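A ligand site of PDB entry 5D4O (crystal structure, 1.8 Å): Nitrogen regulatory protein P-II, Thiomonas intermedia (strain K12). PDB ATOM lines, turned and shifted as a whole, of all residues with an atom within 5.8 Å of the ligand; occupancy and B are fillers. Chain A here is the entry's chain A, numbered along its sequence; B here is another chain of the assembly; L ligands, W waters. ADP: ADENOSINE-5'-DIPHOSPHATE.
OH of Tyr 51 lies within hydrogen-bond range of OG of Ser 90.
N of Ile 67 of chain B sits at hydrogen-bond distance from O of Thr 37 of chain B, at 2.7 Å.
The side-chain amino group of Lys 105 of chain B lies within hydrogen-bond range of the backbone carbonyl oxygen of Gly 91, at 2.8 Å.
N of Tyr 51 sits at hydrogen-bond distance from O of Gly 44, 2.9 Å away.
The backbone carbonyl oxygen (O) of Tyr 36 of chain B lies within hydrogen-bond range of the backbone NH (N) of Lys 45, at 2.9 Å.
The backbone NH of Ile 15 lies within hydrogen-bond range of the backbone carbonyl oxygen of Val 92 (2.9 Å).
The side-chain hydroxyl of Ser 90 sits at hydrogen-bond distance from an oxygen (O1B) of the ligand.
The backbone NH (N) of Ser 47 sits at hydrogen-bond distance from an oxygen (O1A) of the ligand (2.9 Å).
OG of Ser 47 is in hydrogen-bond range of O3B of the ligand, at 2.5 Å.
OG1 of Thr 37 of chain B lies within hydrogen-bond range of O2' of the ligand, at 2.6 Å.
O2A of the ligand is in salt-bridge range of NZ of Lys 105 of chain B, 2.8 Å away.
The backbone NH of Gly 91 is in hydrogen-bond range of an oxygen (O2A) of the ligand (2.9 Å).
N of His 48 is in hydrogen-bond range of O3B of the ligand (2.9 Å).
N of Ala 69 of chain B sits at hydrogen-bond distance from N1 of the ligand (2.9 Å).
The backbone carbonyl oxygen (O) of Ala 69 of chain B lies within hydrogen-bond range of a nitrogen (N6) of the ligand.
OH of Tyr 51 sits at hydrogen-bond distance from O1B of the ligand (3.1 Å).
The backbone carbonyl oxygen (O) of Gly 35 of chain B sits at hydrogen-bond distance from a nitrogen (N6) of the ligand (3.2 Å).
O3' of the ligand lies close to O of Gly 44.
Ile 15 touches the ligand.
O of Lys 45 touches C3' of the ligand, 3.3 Å away.
Gly 46 touches the ligand (CA to O5', 3.5 Å).
N of Gly 49 touches O2B of the ligand, 3.6 Å away.
Leu 63 touches the ligand.
Val 92 touches the ligand.
Phe 94 touches the ligand (CZ to C2, 3.6 Å).
Tyr 36 of chain B touches the ligand.
Ile 67 of chain B touches the ligand.
Ala 68 of chain B touches the ligand (CA to N1, 3.7 Å).
CD1 of Phe 106 of chain B touches N6 of the ligand (3.4 Å).
Hydrophobic or aromatic side chains that line the ligand: Ile 15, His 48, Tyr 51, Leu 63, Val 92, Phe 94, Ala 69 of chain B and Phe 106 of chain B.
Of the 28 residues printed, 21 come within 4 Å of the ligand.
The nearest printed residue that does not touch the ligand is Ser 43 (4.3 Å).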
ATOM      1  N   ILE A  15      33.069  27.043   4.486  1.00  0.00           N
ATOM      2  CA  ILE A  15      32.248  25.916   4.044  1.00  0.00           C
ATOM      3  C   ILE A  15      31.770  26.232   2.641  1.00  0.00           C
ATOM      4  O   ILE A  15      31.190  27.291   2.414  1.00  0.00           O
ATOM      5  CB  ILE A  15      31.077  25.655   5.025  1.00  0.00           C
ATOM      6  CG1 ILE A  15      31.641  25.337   6.435  1.00  0.00           C
ATOM      7  CG2 ILE A  15      30.176  24.489   4.508  1.00  0.00           C
ATOM      8  CD1 ILE A  15      30.633  25.474   7.626  1.00  0.00           C
ATOM      9  N   SER A  43      27.482  17.377   5.080  1.00  0.00           N
ATOM     10  CA  SER A  43      26.102  17.595   4.660  1.00  0.00           C
ATOM     11  C   SER A  43      25.695  18.921   5.274  1.00  0.00           C
ATOM     12  O   SER A  43      26.380  19.429   6.164  1.00  0.00           O
ATOM     13  CB  SER A  43      25.177  16.466   5.077  1.00  0.00           C
ATOM     14  OG  SER A  43      25.640  15.279   4.454  1.00  0.00           O
ATOM     15  N   GLY A  44      24.617  19.476   4.787  1.00  0.00           N
ATOM     16  CA  GLY A  44      24.135  20.732   5.340  1.00  0.00           C
ATOM     17  C   GLY A  44      22.862  21.236   4.730  1.00  0.00           C
ATOM     18  O   GLY A  44      22.475  20.826   3.632  1.00  0.00           O
ATOM     19  N   LYS A  45      22.245  22.170   5.436  1.00  0.00           N
ATOM     20  CA  LYS A  45      21.044  22.847   4.966  1.00  0.00           C
ATOM     21  C   LYS A  45      21.456  24.258   4.619  1.00  0.00           C
ATOM     22  O   LYS A  45      22.087  24.948   5.427  1.00  0.00           O
ATOM     23  CB  LYS A  45      19.987  22.871   6.061  1.00  0.00           C
ATOM     24  CG  LYS A  45      18.673  23.491   5.610  1.00  0.00           C
ATOM     25  CD  LYS A  45      17.839  23.990   6.794  1.00  0.00           C
ATOM     26  CE  LYS A  45      16.435  23.428   6.813  1.00  0.00           C
ATOM     27  NZ  LYS A  45      15.676  23.724   5.569  1.00  0.00           N
ATOM     28  N   GLY A  46      21.111  24.662   3.397  1.00  0.00           N
ATOM     29  CA  GLY A  46      21.347  25.991   2.877  1.00  0.00           C
ATOM     30  C   GLY A  46      20.025  26.689   2.611  1.00  0.00           C
ATOM     31  O   GLY A  46      18.958  26.092   2.764  1.00  0.00           O
ATOM     32  N   SER A  47      20.089  27.976   2.217  1.00  0.00           N
ATOM     33  CA  SER A  47      18.914  28.805   1.943  1.00  0.00           C
ATOM     34  C   SER A  47      18.024  28.286   0.787  1.00  0.00           C
ATOM     35  O   SER A  47      16.834  28.621   0.760  1.00  0.00           O
ATOM     36  CB  SER A  47      19.310  30.251   1.675  1.00  0.00           C
ATOM     37  OG  SER A  47      20.095  30.382   0.502  1.00  0.00           O
ATOM     38  N   HIS A  48      18.598  27.486  -0.133  1.00  0.00           N
ATOM     39  CA  HIS A  48      17.906  26.937  -1.308  1.00  0.00           C
ATOM     40  C   HIS A  48      17.907  25.393  -1.418  1.00  0.00           C
ATOM     41  O   HIS A  48      17.751  24.864  -2.528  1.00  0.00           O
ATOM     42  CB  HIS A  48      18.437  27.592  -2.598  1.00  0.00           C
ATOM     43  N   GLY A  49      18.066  24.682  -0.301  1.00  0.00           N
ATOM     44  CA  GLY A  49      18.035  23.224  -0.310  1.00  0.00           C
ATOM     45  C   GLY A  49      19.144  22.530   0.459  1.00  0.00           C
ATOM     46  O   GLY A  49      20.053  23.174   0.980  1.00  0.00           O
ATOM     47  N   MET A  50      19.029  21.205   0.533  1.00  0.00           N
ATOM     48  CA  MET A  50      19.954  20.318   1.227  1.00  0.00           C
ATOM     49  C   MET A  50      21.123  19.892   0.359  1.00  0.00           C
ATOM     50  O   MET A  50      20.972  19.695  -0.848  1.00  0.00           O
ATOM     51  CB  MET A  50      19.226  19.059   1.705  1.00  0.00           C
ATOM     52  CG  MET A  50      18.111  19.322   2.714  1.00  0.00           C
ATOM     53  SD  MET A  50      18.668  20.009   4.300  1.00  0.00           S
ATOM     54  CE  MET A  50      19.849  18.801   4.820  1.00  0.00           C
ATOM     55  N   TYR A  51      22.284  19.705   1.003  1.00  0.00           N
ATOM     56  CA  TYR A  51      23.484  19.158   0.418  1.00  0.00           C
ATOM     57  C   TYR A  51      23.713  17.869   1.215  1.00  0.00           C
ATOM     58  O   TYR A  51      23.832  17.926   2.434  1.00  0.00           O
ATOM     59  CB  TYR A  51      24.687  20.113   0.603  1.00  0.00           C
ATOM     60  CG  TYR A  51      24.609  21.347  -0.258  1.00  0.00           C
ATOM     61  CD1 TYR A  51      23.900  22.472   0.167  1.00  0.00           C
ATOM     62  CD2 TYR A  51      25.245  21.411  -1.490  1.00  0.00           C
ATOM     63  CE1 TYR A  51      23.820  23.614  -0.623  1.00  0.00           C
ATOM     64  CE2 TYR A  51      25.151  22.542  -2.297  1.00  0.00           C
ATOM     65  CZ  TYR A  51      24.450  23.648  -1.850  1.00  0.00           C
ATOM     66  OH  TYR A  51      24.329  24.762  -2.649  1.00  0.00           O
ATOM     67  N   LEU A  63      30.204  18.957  -0.096  1.00  0.00           N
ATOM     68  CA  LEU A  63      30.603  20.146   0.674  1.00  0.00           C
ATOM     69  C   LEU A  63      31.841  19.778   1.476  1.00  0.00           C
ATOM     70  O   LEU A  63      32.024  18.614   1.872  1.00  0.00           O
ATOM     71  CB  LEU A  63      29.526  20.546   1.708  1.00  0.00           C
ATOM     72  CG  LEU A  63      28.294  21.288   1.237  1.00  0.00           C
ATOM     73  CD1 LEU A  63      27.370  21.498   2.434  1.00  0.00           C
ATOM     74  CD2 LEU A  63      28.644  22.645   0.559  1.00  0.00           C
ATOM     75  N   HIS A  89      28.329  32.067  -5.264  1.00  0.00           N
ATOM     76  CA  HIS A  89      28.276  30.638  -4.986  1.00  0.00           C
ATOM     77  C   HIS A  89      27.848  30.363  -3.548  1.00  0.00           C
ATOM     78  O   HIS A  89      27.950  31.238  -2.694  1.00  0.00           O
ATOM     79  CB  HIS A  89      29.635  29.987  -5.250  1.00  0.00           C
ATOM     80  CG  HIS A  89      30.141  30.188  -6.644  1.00  0.00           C
ATOM     81  ND1 HIS A  89      29.670  29.433  -7.696  1.00  0.00           N
ATOM     82  CD2 HIS A  89      31.061  31.066  -7.104  1.00  0.00           C
ATOM     83  CE1 HIS A  89      30.315  29.867  -8.768  1.00  0.00           C
ATOM     84  NE2 HIS A  89      31.171  30.841  -8.461  1.00  0.00           N
ATOM     85  N   SER A  90      27.378  29.140  -3.290  1.00  0.00           N
ATOM     86  CA  SER A  90      26.923  28.725  -1.968  1.00  0.00           C
ATOM     87  C   SER A  90      28.075  28.638  -0.979  1.00  0.00           C
ATOM     88  O   SER A  90      29.220  28.335  -1.339  1.00  0.00           O
ATOM     89  CB  SER A  90      26.231  27.366  -2.068  1.00  0.00           C
ATOM     90  OG  SER A  90      25.074  27.506  -2.866  1.00  0.00           O
ATOM     91  N   GLY A  91      27.737  28.834   0.273  1.00  0.00           N
ATOM     92  CA  GLY A  91      28.737  28.675   1.338  1.00  0.00           C
ATOM     93  C   GLY A  91      28.813  29.833   2.274  1.00  0.00           C
ATOM     94  O   GLY A  91      28.175  30.880   2.072  1.00  0.00           O
ATOM     95  N   VAL A  92      29.613  29.642   3.345  1.00  0.00           N
ATOM     96  CA  VAL A  92      29.740  30.602   4.433  1.00  0.00           C
ATOM     97  C   VAL A  92      31.178  30.614   4.996  1.00  0.00           C
ATOM     98  O   VAL A  92      31.929  29.662   4.793  1.00  0.00           O
ATOM     99  CB  VAL A  92      28.705  30.286   5.578  1.00  0.00           C
ATOM    100  CG1 VAL A  92      27.254  30.515   5.110  1.00  0.00           C
ATOM    101  CG2 VAL A  92      28.875  28.872   6.132  1.00  0.00           C
ATOM    102  N   PHE A  94      33.101  31.522   8.768  1.00  0.00           N
ATOM    103  CA  PHE A  94      32.956  31.895  10.160  1.00  0.00           C
ATOM    104  C   PHE A  94      34.340  32.270  10.692  1.00  0.00           C
ATOM    105  O   PHE A  94      35.282  31.489  10.541  1.00  0.00           O
ATOM    106  CB  PHE A  94      32.399  30.737  10.998  1.00  0.00           C
ATOM    107  CG  PHE A  94      31.106  30.144  10.502  1.00  0.00           C
ATOM    108  CD1 PHE A  94      30.078  30.953  10.014  1.00  0.00           C
ATOM    109  CD2 PHE A  94      30.880  28.771  10.560  1.00  0.00           C
ATOM    110  CE1 PHE A  94      28.877  30.397   9.543  1.00  0.00           C
ATOM    111  CE2 PHE A  94      29.672  28.219  10.110  1.00  0.00           C
ATOM    112  CZ  PHE A  94      28.676  29.032   9.628  1.00  0.00           C
ATOM    113  N   VAL B  33      16.538  28.564  13.021  1.00  0.00           N
ATOM    114  CA  VAL B  33      17.924  28.620  12.528  1.00  0.00           C
ATOM    115  C   VAL B  33      17.945  28.475  10.996  1.00  0.00           C
ATOM    116  O   VAL B  33      17.212  27.657  10.434  1.00  0.00           O
ATOM    117  CB  VAL B  33      19.062  27.922  13.339  1.00  0.00           C
ATOM    118  CG1 VAL B  33      18.620  27.406  14.691  1.00  0.00           C
ATOM    119  CG2 VAL B  33      19.838  26.896  12.530  1.00  0.00           C
ATOM    120  N   LYS B  34      18.695  29.350  10.320  1.00  0.00           N
ATOM    121  CA  LYS B  34      18.679  29.454   8.858  1.00  0.00           C
ATOM    122  C   LYS B  34      19.448  28.365   8.108  1.00  0.00           C
ATOM    123  O   LYS B  34      19.150  28.097   6.950  1.00  0.00           O
ATOM    124  CB  LYS B  34      19.135  30.858   8.446  1.00  0.00           C
ATOM    125  CG  LYS B  34      18.111  31.931   8.792  1.00  0.00           C
ATOM    126  CD  LYS B  34      17.417  32.441   7.547  1.00  0.00           C
ATOM    127  CE  LYS B  34      16.913  33.848   7.741  1.00  0.00           C
ATOM    128  NZ  LYS B  34      18.027  34.788   7.989  1.00  0.00           N
ATOM    129  N   GLY B  35      20.395  27.764   8.770  1.00  0.00           N
ATOM    130  CA  GLY B  35      21.229  26.732   8.158  1.00  0.00           C
ATOM    131  C   GLY B  35      22.040  25.977   9.181  1.00  0.00           C
ATOM    132  O   GLY B  35      22.081  26.364  10.361  1.00  0.00           O
ATOM    133  N   TYR B  36      22.685  24.902   8.727  1.00  0.00           N
ATOM    134  CA  TYR B  36      23.526  24.094   9.608  1.00  0.00           C
ATOM    135  C   TYR B  36      24.402  23.209   8.748  1.00  0.00           C
ATOM    136  O   TYR B  36      24.081  22.941   7.586  1.00  0.00           O
ATOM    137  CB  TYR B  36      22.700  23.256  10.626  1.00  0.00           C
ATOM    138  CG  TYR B  36      21.672  22.333   9.998  1.00  0.00           C
ATOM    139  CD1 TYR B  36      22.062  21.141   9.384  1.00  0.00           C
ATOM    140  CD2 TYR B  36      20.320  22.616  10.084  1.00  0.00           C
ATOM    141  CE1 TYR B  36      21.119  20.294   8.806  1.00  0.00           C
ATOM    142  CE2 TYR B  36      19.363  21.768   9.510  1.00  0.00           C
ATOM    143  CZ  TYR B  36      19.773  20.613   8.866  1.00  0.00           C
ATOM    144  OH  TYR B  36      18.854  19.782   8.293  1.00  0.00           O
ATOM    145  N   THR B  37      25.526  22.798   9.304  1.00  0.00           N
ATOM    146  CA  THR B  37      26.493  21.930   8.647  1.00  0.00           C
ATOM    147  C   THR B  37      26.689  20.689   9.500  1.00  0.00           C
ATOM    148  O   THR B  37      26.878  20.793  10.705  1.00  0.00           O
ATOM    149  CB  THR B  37      27.821  22.671   8.370  1.00  0.00           C
ATOM    150  OG1 THR B  37      27.591  23.723   7.418  1.00  0.00           O
ATOM    151  CG2 THR B  37      28.910  21.727   7.836  1.00  0.00           C
ATOM    152  N   ILE B  38      26.654  19.518   8.858  1.00  0.00           N
ATOM    153  CA  ILE B  38      26.814  18.258   9.594  1.00  0.00           C
ATOM    154  C   ILE B  38      28.122  17.587   9.234  1.00  0.00           C
ATOM    155  O   ILE B  38      28.326  17.211   8.082  1.00  0.00           O
ATOM    156  CB  ILE B  38      25.603  17.290   9.429  1.00  0.00           C
ATOM    157  CG1 ILE B  38      24.244  18.033   9.692  1.00  0.00           C
ATOM    158  CG2 ILE B  38      25.790  16.037  10.358  1.00  0.00           C
ATOM    159  CD1 ILE B  38      23.005  17.239   9.455  1.00  0.00           C
ATOM    160  N   ILE B  67      27.060  21.875  13.164  1.00  0.00           N
ATOM    161  CA  ILE B  67      27.605  23.240  13.297  1.00  0.00           C
ATOM    162  C   ILE B  67      26.481  24.149  12.879  1.00  0.00           C
ATOM    163  O   ILE B  67      25.980  24.044  11.750  1.00  0.00           O
ATOM    164  CB  ILE B  67      28.858  23.474  12.414  1.00  0.00           C
ATOM    165  CG1 ILE B  67      30.014  22.499  12.774  1.00  0.00           C
ATOM    166  CG2 ILE B  67      29.305  24.959  12.510  1.00  0.00           C
ATOM    167  CD1 ILE B  67      31.085  22.423  11.671  1.00  0.00           C
ATOM    168  N   ALA B  68      26.084  25.058  13.773  1.00  0.00           N
ATOM    169  CA  ALA B  68      25.003  25.982  13.450  1.00  0.00           C
ATOM    170  C   ALA B  68      25.339  27.414  13.876  1.00  0.00           C
ATOM    171  O   ALA B  68      25.451  27.687  15.081  1.00  0.00           O
ATOM    172  CB  ALA B  68      23.687  25.502  14.095  1.00  0.00           C
ATOM    173  N   ALA B  69      25.512  28.335  12.890  1.00  0.00           N
ATOM    174  CA  ALA B  69      25.725  29.756  13.186  1.00  0.00           C
ATOM    175  C   ALA B  69      24.333  30.348  13.396  1.00  0.00           C
ATOM    176  O   ALA B  69      23.444  30.165  12.539  1.00  0.00           O
ATOM    177  CB  ALA B  69      26.450  30.444  12.031  1.00  0.00           C
ATOM    178  N   VAL B  70      24.120  30.982  14.573  1.00  0.00           N
ATOM    179  CA  VAL B  70      22.814  31.504  14.994  1.00  0.00           C
ATOM    180  C   VAL B  70      22.941  32.898  15.648  1.00  0.00           C
ATOM    181  O   VAL B  70      23.962  33.179  16.275  1.00  0.00           O
ATOM    182  CB  VAL B  70      22.137  30.503  16.004  1.00  0.00           C
ATOM    183  CG1 VAL B  70      21.939  29.113  15.382  1.00  0.00           C
ATOM    184  CG2 VAL B  70      22.919  30.369  17.314  1.00  0.00           C
ATOM    185  N   LYS B 105      22.058  36.616   6.493  1.00  0.00           N
ATOM    186  CA  LYS B 105      21.987  35.226   6.073  1.00  0.00           C
ATOM    187  C   LYS B 105      21.677  34.332   7.261  1.00  0.00           C
ATOM    188  O   LYS B 105      21.249  33.189   7.086  1.00  0.00           O
ATOM    189  CB  LYS B 105      23.324  34.802   5.435  1.00  0.00           C
ATOM    190  CG  LYS B 105      23.195  33.609   4.516  1.00  0.00           C
ATOM    191  CD  LYS B 105      24.503  33.208   3.881  1.00  0.00           C
ATOM    192  CE  LYS B 105      24.314  31.929   3.104  1.00  0.00           C
ATOM    193  NZ  LYS B 105      25.515  31.603   2.284  1.00  0.00           N
ATOM    194  N   PHE B 106      21.929  34.827   8.486  1.00  0.00           N
ATOM    195  CA  PHE B 106      21.790  33.988   9.671  1.00  0.00           C
ATOM    196  C   PHE B 106      20.668  34.355  10.623  1.00  0.00           C
ATOM    197  O   PHE B 106      20.291  33.513  11.451  1.00  0.00           O
ATOM    198  CB  PHE B 106      23.140  33.889  10.419  1.00  0.00           C
ATOM    199  CG  PHE B 106      24.329  33.603   9.529  1.00  0.00           C
ATOM    200  CD1 PHE B 106      24.687  32.290   9.209  1.00  0.00           C
ATOM    201  CD2 PHE B 106      25.087  34.642   8.982  1.00  0.00           C
ATOM    202  CE1 PHE B 106      25.760  32.021   8.351  1.00  0.00           C
ATOM    203  CE2 PHE B 106      26.184  34.365   8.149  1.00  0.00           C
ATOM    204  CZ  PHE B 106      26.510  33.064   7.825  1.00  0.00           C
HETATM  205  PB  ADP L   1      22.131  27.357  -0.942  1.00  0.00           P
HETATM  206  O1B ADP L   1      22.673  27.362  -2.288  1.00  0.00           O
HETATM  207  O2B ADP L   1      21.339  26.062  -0.723  1.00  0.00           O
HETATM  208  O3B ADP L   1      21.243  28.542  -0.715  1.00  0.00           O
HETATM  209  PA  ADP L   1      23.877  28.354   1.317  1.00  0.00           P
HETATM  210  O1A ADP L   1      22.802  29.092   2.025  1.00  0.00           O
HETATM  211  O2A ADP L   1      24.938  29.298   0.794  1.00  0.00           O
HETATM  212  O3A ADP L   1      23.344  27.433   0.113  1.00  0.00           O
HETATM  213  O5' ADP L   1      24.518  27.323   2.341  1.00  0.00           O
HETATM  214  C5' ADP L   1      25.485  26.377   1.866  1.00  0.00           C
HETATM  215  C4' ADP L   1      26.009  25.563   3.030  1.00  0.00           C
HETATM  216  O4' ADP L   1      26.603  26.431   4.010  1.00  0.00           O
HETATM  217  C3' ADP L   1      24.959  24.789   3.813  1.00  0.00           C
HETATM  218  O3' ADP L   1      24.592  23.576   3.190  1.00  0.00           O
HETATM  219  C2' ADP L   1      25.686  24.568   5.136  1.00  0.00           C
HETATM  220  O2' ADP L   1      26.635  23.520   4.995  1.00  0.00           O
HETATM  221  C1' ADP L   1      26.421  25.891   5.312  1.00  0.00           C
HETATM  222  N9  ADP L   1      25.695  26.841   6.131  1.00  0.00           N
HETATM  223  C8  ADP L   1      24.805  27.804   5.714  1.00  0.00           C
HETATM  224  N7  ADP L   1      24.238  28.466   6.689  1.00  0.00           N
HETATM  225  C5  ADP L   1      24.782  27.903   7.833  1.00  0.00           C
HETATM  226  C6  ADP L   1      24.603  28.167   9.211  1.00  0.00           C
HETATM  227  N6  ADP L   1      23.694  29.032   9.676  1.00  0.00           N
HETATM  228  N1  ADP L   1      25.337  27.448  10.087  1.00  0.00           N
HETATM  229  C2  ADP L   1      26.148  26.492   9.620  1.00  0.00           C
HETATM  230  N3  ADP L   1      26.371  26.125   8.357  1.00  0.00           N
HETATM  231  C4  ADP L   1      25.682  26.900   7.500  1.00  0.00           C
HETATM  232  O   HOH W   1      22.064  29.827   4.595  1.00  0.00           O
